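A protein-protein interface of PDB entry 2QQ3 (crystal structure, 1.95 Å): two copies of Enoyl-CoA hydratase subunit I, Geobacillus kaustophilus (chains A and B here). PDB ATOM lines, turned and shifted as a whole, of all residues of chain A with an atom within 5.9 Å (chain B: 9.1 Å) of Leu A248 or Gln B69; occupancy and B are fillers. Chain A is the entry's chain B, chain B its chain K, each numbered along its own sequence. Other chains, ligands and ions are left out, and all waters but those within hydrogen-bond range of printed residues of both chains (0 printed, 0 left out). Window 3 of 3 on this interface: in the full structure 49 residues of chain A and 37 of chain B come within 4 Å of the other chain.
Of the 8 printed residues of chain A, 4 touch a printed residue of chain B.
Hydrophobic or aromatic side chains of chain A within 4 Å of the printed part of chain B: Met A244, Phe A247 and Leu A248.
Along chain A the printed residues that touch a printed residue of chain B span positions 243 to 248.
Printed residues of chain B that touch a printed residue of chain A: Ile B68, Gln B69, Met B71, Ala B72 and Leu B135.
The backbone NH (N) of Gln B69 sits at hydrogen-bond distance from the side-chain carboxylate (OD1) of Asp B67 (3.2 Å).
No position is printed for both chains.
Of the 10 pairs that touch across the chains among the printed residues, none has its exchanged pair printed and touching as well.
Of chain B, only Ile B68, Gln B69 and Ala B72 come within 4 Å of Leu A248.
Of chain A, only Leu A248 (3.4 Å) comes within 4 Å of Gln B69.
Of the printed residues of chain B, Phe A247 touches Ile B68 and Leu B135.
Of the printed residues of chain A, Met B71 touches Met A244.
Ala B66 touches none of the printed residues of chain A.
Ala B28 touches none of the printed residues of chain A.
The nearest printed residue of chain A that does not touch Gln B69 is Phe A247 (6.4 Å).
The nearest printed residue of chain B that does not touch Met A244 is Lys B73 (5.8 Å).
Gly A243 touches Leu B135.
CB of Met A244 touches CG2 of Ile B68, 3.8 Å away.
CE of Met A244 touches SD of Met B71, at 3.99 Å.
Ala B72 touches Met A244 (CA to SD, 3.8 Å).
Met A244 touches Leu B135 (N to O, 3.6 Å).
Phe A247 touches Ile B68 (CE2 to CG1, 3.5 Å).
Leu B135 touches Phe A247.
Leu A248 touches Ile B68.
Gln B69 touches Leu A248.
Ala B72 touches Leu A248 (CB to CD1, 3.7 Å).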
ATOM      1  N   GLY A 243     -18.471 -25.216   5.471  1.00  0.00           N
ATOM      2  CA  GLY A 243     -17.048 -25.404   5.704  1.00  0.00           C
ATOM      3  C   GLY A 243     -16.184 -24.418   4.938  1.00  0.00           C
ATOM      4  O   GLY A 243     -15.223 -23.870   5.479  1.00  0.00           O
ATOM      5  N   MET A 244     -16.525 -24.184   3.677  1.00  0.00           N
ATOM      6  CA  MET A 244     -15.756 -23.260   2.860  1.00  0.00           C
ATOM      7  C   MET A 244     -16.098 -21.809   3.160  1.00  0.00           C
ATOM      8  O   MET A 244     -15.220 -20.949   3.156  1.00  0.00           O
ATOM      9  CB  MET A 244     -15.962 -23.577   1.379  1.00  0.00           C
ATOM     10  CG  MET A 244     -15.411 -24.951   1.011  1.00  0.00           C
ATOM     11  SD  MET A 244     -15.327 -25.255  -0.750  1.00  0.00           S
ATOM     12  CE  MET A 244     -14.407 -26.847  -0.778  1.00  0.00           C
ATOM     13  N   ALA A 245     -17.369 -21.537   3.429  1.00  0.00           N
ATOM     14  CA  ALA A 245     -17.781 -20.179   3.755  1.00  0.00           C
ATOM     15  C   ALA A 245     -17.048 -19.759   5.029  1.00  0.00           C
ATOM     16  O   ALA A 245     -16.505 -18.657   5.110  1.00  0.00           O
ATOM     17  CB  ALA A 245     -19.291 -20.121   3.971  1.00  0.00           C
ATOM     18  N   ALA A 246     -17.024 -20.653   6.015  1.00  0.00           N
ATOM     19  CA  ALA A 246     -16.355 -20.381   7.284  1.00  0.00           C
ATOM     20  C   ALA A 246     -14.865 -20.107   7.080  1.00  0.00           C
ATOM     21  O   ALA A 246     -14.300 -19.186   7.673  1.00  0.00           O
ATOM     22  CB  ALA A 246     -16.544 -21.560   8.235  1.00  0.00           C
ATOM     23  N   PHE A 247     -14.236 -20.914   6.234  1.00  0.00           N
ATOM     24  CA  PHE A 247     -12.813 -20.777   5.941  1.00  0.00           C
ATOM     25  C   PHE A 247     -12.496 -19.402   5.362  1.00  0.00           C
ATOM     26  O   PHE A 247     -11.493 -18.782   5.723  1.00  0.00           O
ATOM     27  CB  PHE A 247     -12.391 -21.854   4.943  1.00  0.00           C
ATOM     28  CG  PHE A 247     -10.961 -21.748   4.496  1.00  0.00           C
ATOM     29  CD1 PHE A 247      -9.924 -22.197   5.307  1.00  0.00           C
ATOM     30  CD2 PHE A 247     -10.652 -21.207   3.253  1.00  0.00           C
ATOM     31  CE1 PHE A 247      -8.596 -22.112   4.884  1.00  0.00           C
ATOM     32  CE2 PHE A 247      -9.332 -21.115   2.820  1.00  0.00           C
ATOM     33  CZ  PHE A 247      -8.302 -21.570   3.635  1.00  0.00           C
ATOM     34  N   LEU A 248     -13.354 -18.940   4.457  1.00  0.00           N
ATOM     35  CA  LEU A 248     -13.178 -17.644   3.803  1.00  0.00           C
ATOM     36  C   LEU A 248     -13.619 -16.476   4.682  1.00  0.00           C
ATOM     37  O   LEU A 248     -13.275 -15.327   4.412  1.00  0.00           O
ATOM     38  CB  LEU A 248     -13.971 -17.603   2.492  1.00  0.00           C
ATOM     39  CG  LEU A 248     -13.678 -18.668   1.430  1.00  0.00           C
ATOM     40  CD1 LEU A 248     -14.642 -18.494   0.258  1.00  0.00           C
ATOM     41  CD2 LEU A 248     -12.234 -18.552   0.962  1.00  0.00           C
ATOM     42  N   GLU A 249     -14.384 -16.771   5.727  1.00  0.00           N
ATOM     43  CA  GLU A 249     -14.870 -15.738   6.633  1.00  0.00           C
ATOM     44  C   GLU A 249     -14.162 -15.779   7.982  1.00  0.00           C
ATOM     45  O   GLU A 249     -14.588 -15.125   8.933  1.00  0.00           O
ATOM     46  CB  GLU A 249     -16.379 -15.893   6.829  1.00  0.00           C
ATOM     47  CG  GLU A 249     -17.203 -15.356   5.671  1.00  0.00           C
ATOM     48  CD  GLU A 249     -18.604 -15.925   5.632  1.00  0.00           C
ATOM     49  OE1 GLU A 249     -19.214 -16.086   6.709  1.00  0.00           O
ATOM     50  OE2 GLU A 249     -19.104 -16.206   4.521  1.00  0.00           O
ATOM     51  N   LYS A 250     -13.074 -16.542   8.052  1.00  0.00           N
ATOM     52  CA  LYS A 250     -12.296 -16.684   9.280  1.00  0.00           C
ATOM     53  C   LYS A 250     -13.204 -16.881  10.494  1.00  0.00           C
ATOM     54  O   LYS A 250     -13.109 -16.136  11.471  1.00  0.00           O
ATOM     55  CB  LYS A 250     -11.418 -15.449   9.527  1.00  0.00           C
ATOM     56  CG  LYS A 250     -10.624 -14.936   8.333  1.00  0.00           C
ATOM     57  CD  LYS A 250     -11.504 -14.120   7.398  1.00  0.00           C
ATOM     58  CE  LYS A 250     -10.683 -13.343   6.377  1.00  0.00           C
ATOM     59  NZ  LYS A 250      -9.915 -12.224   6.992  1.00  0.00           N
ATOM     60  N   ALA B  28      -1.532 -20.824  -3.591  1.00  0.00           N
ATOM     61  CA  ALA B  28      -2.781 -21.582  -3.561  1.00  0.00           C
ATOM     62  C   ALA B  28      -3.049 -22.068  -4.977  1.00  0.00           C
ATOM     63  O   ALA B  28      -3.002 -21.282  -5.922  1.00  0.00           O
ATOM     64  CB  ALA B  28      -3.927 -20.700  -3.088  1.00  0.00           C
ATOM     65  N   LEU B  29      -3.327 -23.360  -5.131  1.00  0.00           N
ATOM     66  CA  LEU B  29      -3.577 -23.918  -6.458  1.00  0.00           C
ATOM     67  C   LEU B  29      -4.971 -23.655  -7.015  1.00  0.00           C
ATOM     68  O   LEU B  29      -5.946 -24.282  -6.604  1.00  0.00           O
ATOM     69  CB  LEU B  29      -3.333 -25.432  -6.459  1.00  0.00           C
ATOM     70  CG  LEU B  29      -1.920 -25.938  -6.179  1.00  0.00           C
ATOM     71  CD1 LEU B  29      -1.934 -27.458  -6.170  1.00  0.00           C
ATOM     72  CD2 LEU B  29      -0.950 -25.416  -7.238  1.00  0.00           C
ATOM     73  N   SER B  30      -5.065 -22.733  -7.964  1.00  0.00           N
ATOM     74  CA  SER B  30      -6.342 -22.438  -8.592  1.00  0.00           C
ATOM     75  C   SER B  30      -6.439 -23.346  -9.811  1.00  0.00           C
ATOM     76  O   SER B  30      -5.444 -23.948 -10.222  1.00  0.00           O
ATOM     77  CB  SER B  30      -6.396 -20.984  -9.048  1.00  0.00           C
ATOM     78  OG  SER B  30      -5.487 -20.768 -10.112  1.00  0.00           O
ATOM     79  N   ARG B  31      -7.630 -23.444 -10.391  1.00  0.00           N
ATOM     80  CA  ARG B  31      -7.817 -24.273 -11.571  1.00  0.00           C
ATOM     81  C   ARG B  31      -7.027 -23.681 -12.732  1.00  0.00           C
ATOM     82  O   ARG B  31      -6.549 -24.404 -13.607  1.00  0.00           O
ATOM     83  CB  ARG B  31      -9.309 -24.380 -11.899  1.00  0.00           C
ATOM     84  CG  ARG B  31     -10.032 -25.315 -10.937  1.00  0.00           C
ATOM     85  CD  ARG B  31     -11.507 -25.498 -11.254  1.00  0.00           C
ATOM     86  NE  ARG B  31     -12.336 -24.454 -10.670  1.00  0.00           N
ATOM     87  CZ  ARG B  31     -13.372 -24.676  -9.865  1.00  0.00           C
ATOM     88  NH1 ARG B  31     -13.716 -25.913  -9.534  1.00  0.00           N
ATOM     89  NH2 ARG B  31     -14.067 -23.653  -9.393  1.00  0.00           N
ATOM     90  N   ALA B  66      -5.723 -25.176  -2.197  1.00  0.00           N
ATOM     91  CA  ALA B  66      -6.213 -24.725  -3.485  1.00  0.00           C
ATOM     92  C   ALA B  66      -6.968 -23.425  -3.278  1.00  0.00           C
ATOM     93  O   ALA B  66      -7.095 -22.944  -2.154  1.00  0.00           O
ATOM     94  CB  ALA B  66      -7.133 -25.781  -4.093  1.00  0.00           C
ATOM     95  N   ASP B  67      -7.455 -22.852  -4.371  1.00  0.00           N
ATOM     96  CA  ASP B  67      -8.214 -21.611  -4.305  1.00  0.00           C
ATOM     97  C   ASP B  67      -9.624 -21.985  -3.868  1.00  0.00           C
ATOM     98  O   ASP B  67     -10.384 -22.562  -4.643  1.00  0.00           O
ATOM     99  CB  ASP B  67      -8.253 -20.947  -5.682  1.00  0.00           C
ATOM    100  CG  ASP B  67      -8.876 -19.566  -5.646  1.00  0.00           C
ATOM    101  OD1 ASP B  67     -10.053 -19.449  -5.235  1.00  0.00           O
ATOM    102  OD2 ASP B  67      -8.183 -18.600  -6.033  1.00  0.00           O
ATOM    103  N   ILE B  68      -9.968 -21.662  -2.627  1.00  0.00           N
ATOM    104  CA  ILE B  68     -11.283 -21.993  -2.099  1.00  0.00           C
ATOM    105  C   ILE B  68     -12.399 -21.098  -2.627  1.00  0.00           C
ATOM    106  O   ILE B  68     -13.508 -21.564  -2.883  1.00  0.00           O
ATOM    107  CB  ILE B  68     -11.285 -21.934  -0.551  1.00  0.00           C
ATOM    108  CG1 ILE B  68     -10.237 -22.904   0.008  1.00  0.00           C
ATOM    109  CG2 ILE B  68     -12.673 -22.263  -0.014  1.00  0.00           C
ATOM    110  CD1 ILE B  68     -10.335 -24.320  -0.543  1.00  0.00           C
ATOM    111  N   GLN B  69     -12.105 -19.813  -2.786  1.00  0.00           N
ATOM    112  CA  GLN B  69     -13.097 -18.863  -3.275  1.00  0.00           C
ATOM    113  C   GLN B  69     -13.765 -19.275  -4.587  1.00  0.00           C
ATOM    114  O   GLN B  69     -14.983 -19.192  -4.724  1.00  0.00           O
ATOM    115  CB  GLN B  69     -12.457 -17.484  -3.454  1.00  0.00           C
ATOM    116  CG  GLN B  69     -13.412 -16.439  -4.006  1.00  0.00           C
ATOM    117  CD  GLN B  69     -14.647 -16.277  -3.142  1.00  0.00           C
ATOM    118  OE1 GLN B  69     -14.554 -15.930  -1.964  1.00  0.00           O
ATOM    119  NE2 GLN B  69     -15.815 -16.533  -3.724  1.00  0.00           N
ATOM    120  N   GLU B  70     -12.968 -19.726  -5.550  1.00  0.00           N
ATOM    121  CA  GLU B  70     -13.512 -20.104  -6.843  1.00  0.00           C
ATOM    122  C   GLU B  70     -14.404 -21.343  -6.826  1.00  0.00           C
ATOM    123  O   GLU B  70     -15.104 -21.603  -7.802  1.00  0.00           O
ATOM    124  CB  GLU B  70     -12.380 -20.285  -7.864  1.00  0.00           C
ATOM    125  CG  GLU B  70     -11.643 -21.617  -7.782  1.00  0.00           C
ATOM    126  CD  GLU B  70     -10.536 -21.720  -8.816  1.00  0.00           C
ATOM    127  OE1 GLU B  70     -10.636 -21.037  -9.857  1.00  0.00           O
ATOM    128  OE2 GLU B  70      -9.577 -22.488  -8.596  1.00  0.00           O
ATOM    129  N   MET B  71     -14.395 -22.105  -5.734  1.00  0.00           N
ATOM    130  CA  MET B  71     -15.240 -23.302  -5.675  1.00  0.00           C
ATOM    131  C   MET B  71     -16.172 -23.329  -4.468  1.00  0.00           C
ATOM    132  O   MET B  71     -16.962 -24.265  -4.305  1.00  0.00           O
ATOM    133  CB  MET B  71     -14.376 -24.578  -5.690  1.00  0.00           C
ATOM    134  CG  MET B  71     -13.647 -24.901  -4.384  1.00  0.00           C
ATOM    135  SD  MET B  71     -12.798 -26.524  -4.414  1.00  0.00           S
ATOM    136  CE  MET B  71     -11.191 -26.067  -3.844  1.00  0.00           C
ATOM    137  N   ALA B  72     -16.100 -22.295  -3.634  1.00  0.00           N
ATOM    138  CA  ALA B  72     -16.929 -22.229  -2.432  1.00  0.00           C
ATOM    139  C   ALA B  72     -18.428 -22.404  -2.681  1.00  0.00           C
ATOM    140  O   ALA B  72     -19.141 -22.941  -1.834  1.00  0.00           O
ATOM    141  CB  ALA B  72     -16.671 -20.917  -1.694  1.00  0.00           C
ATOM    142  N   LYS B  73     -18.911 -21.961  -3.835  1.00  0.00           N
ATOM    143  CA  LYS B  73     -20.335 -22.086  -4.150  1.00  0.00           C
ATOM    144  C   LYS B  73     -20.646 -23.122  -5.234  1.00  0.00           C
ATOM    145  O   LYS B  73     -21.737 -23.120  -5.795  1.00  0.00           O
ATOM    146  CB  LYS B  73     -20.895 -20.734  -4.593  1.00  0.00           C
ATOM    147  CG  LYS B  73     -20.757 -19.619  -3.572  1.00  0.00           C
ATOM    148  CD  LYS B  73     -21.828 -19.693  -2.501  1.00  0.00           C
ATOM    149  CE  LYS B  73     -21.829 -18.431  -1.646  1.00  0.00           C
ATOM    150  NZ  LYS B  73     -22.981 -18.389  -0.704  1.00  0.00           N
ATOM    151  N   ASP B  74     -19.700 -24.006  -5.535  1.00  0.00           N
ATOM    152  CA  ASP B  74     -19.941 -25.009  -6.565  1.00  0.00           C
ATOM    153  C   ASP B  74     -20.989 -26.050  -6.191  1.00  0.00           C
ATOM    154  O   ASP B  74     -21.337 -26.213  -5.023  1.00  0.00           O
ATOM    155  CB  ASP B  74     -18.635 -25.715  -6.936  1.00  0.00           C
ATOM    156  CG  ASP B  74     -17.683 -24.809  -7.689  1.00  0.00           C
ATOM    157  OD1 ASP B  74     -18.131 -23.740  -8.147  1.00  0.00           O
ATOM    158  OD2 ASP B  74     -16.495 -25.167  -7.829  1.00  0.00           O
ATOM    159  N   ARG B  78     -22.097 -28.517 -11.820  1.00  0.00           N
ATOM    160  CA  ARG B  78     -21.047 -27.687 -12.397  1.00  0.00           C
ATOM    161  C   ARG B  78     -19.731 -28.461 -12.454  1.00  0.00           C
ATOM    162  O   ARG B  78     -19.043 -28.461 -13.476  1.00  0.00           O
ATOM    163  CB  ARG B  78     -20.816 -26.413 -11.582  1.00  0.00           C
ATOM    164  CG  ARG B  78     -19.776 -25.518 -12.246  1.00  0.00           C
ATOM    165  CD  ARG B  78     -19.054 -24.583 -11.290  1.00  0.00           C
ATOM    166  NE  ARG B  78     -17.969 -23.901 -11.992  1.00  0.00           N
ATOM    167  CZ  ARG B  78     -17.103 -23.065 -11.429  1.00  0.00           C
ATOM    168  NH1 ARG B  78     -17.178 -22.790 -10.137  1.00  0.00           N
ATOM    169  NH2 ARG B  78     -16.152 -22.503 -12.166  1.00  0.00           N
ATOM    170  N   LEU B 135     -12.971 -28.595   5.770  1.00  0.00           N
ATOM    171  CA  LEU B 135     -13.716 -27.659   4.934  1.00  0.00           C
ATOM    172  C   LEU B 135     -15.027 -28.307   4.502  1.00  0.00           C
ATOM    173  O   LEU B 135     -15.787 -27.737   3.723  1.00  0.00           O
ATOM    174  CB  LEU B 135     -12.906 -27.278   3.697  1.00  0.00           C
ATOM    175  CG  LEU B 135     -11.810 -26.239   3.926  1.00  0.00           C
ATOM    176  CD1 LEU B 135     -10.980 -26.045   2.669  1.00  0.00           C
ATOM    177  CD2 LEU B 135     -12.464 -24.944   4.325  1.00  0.00           C
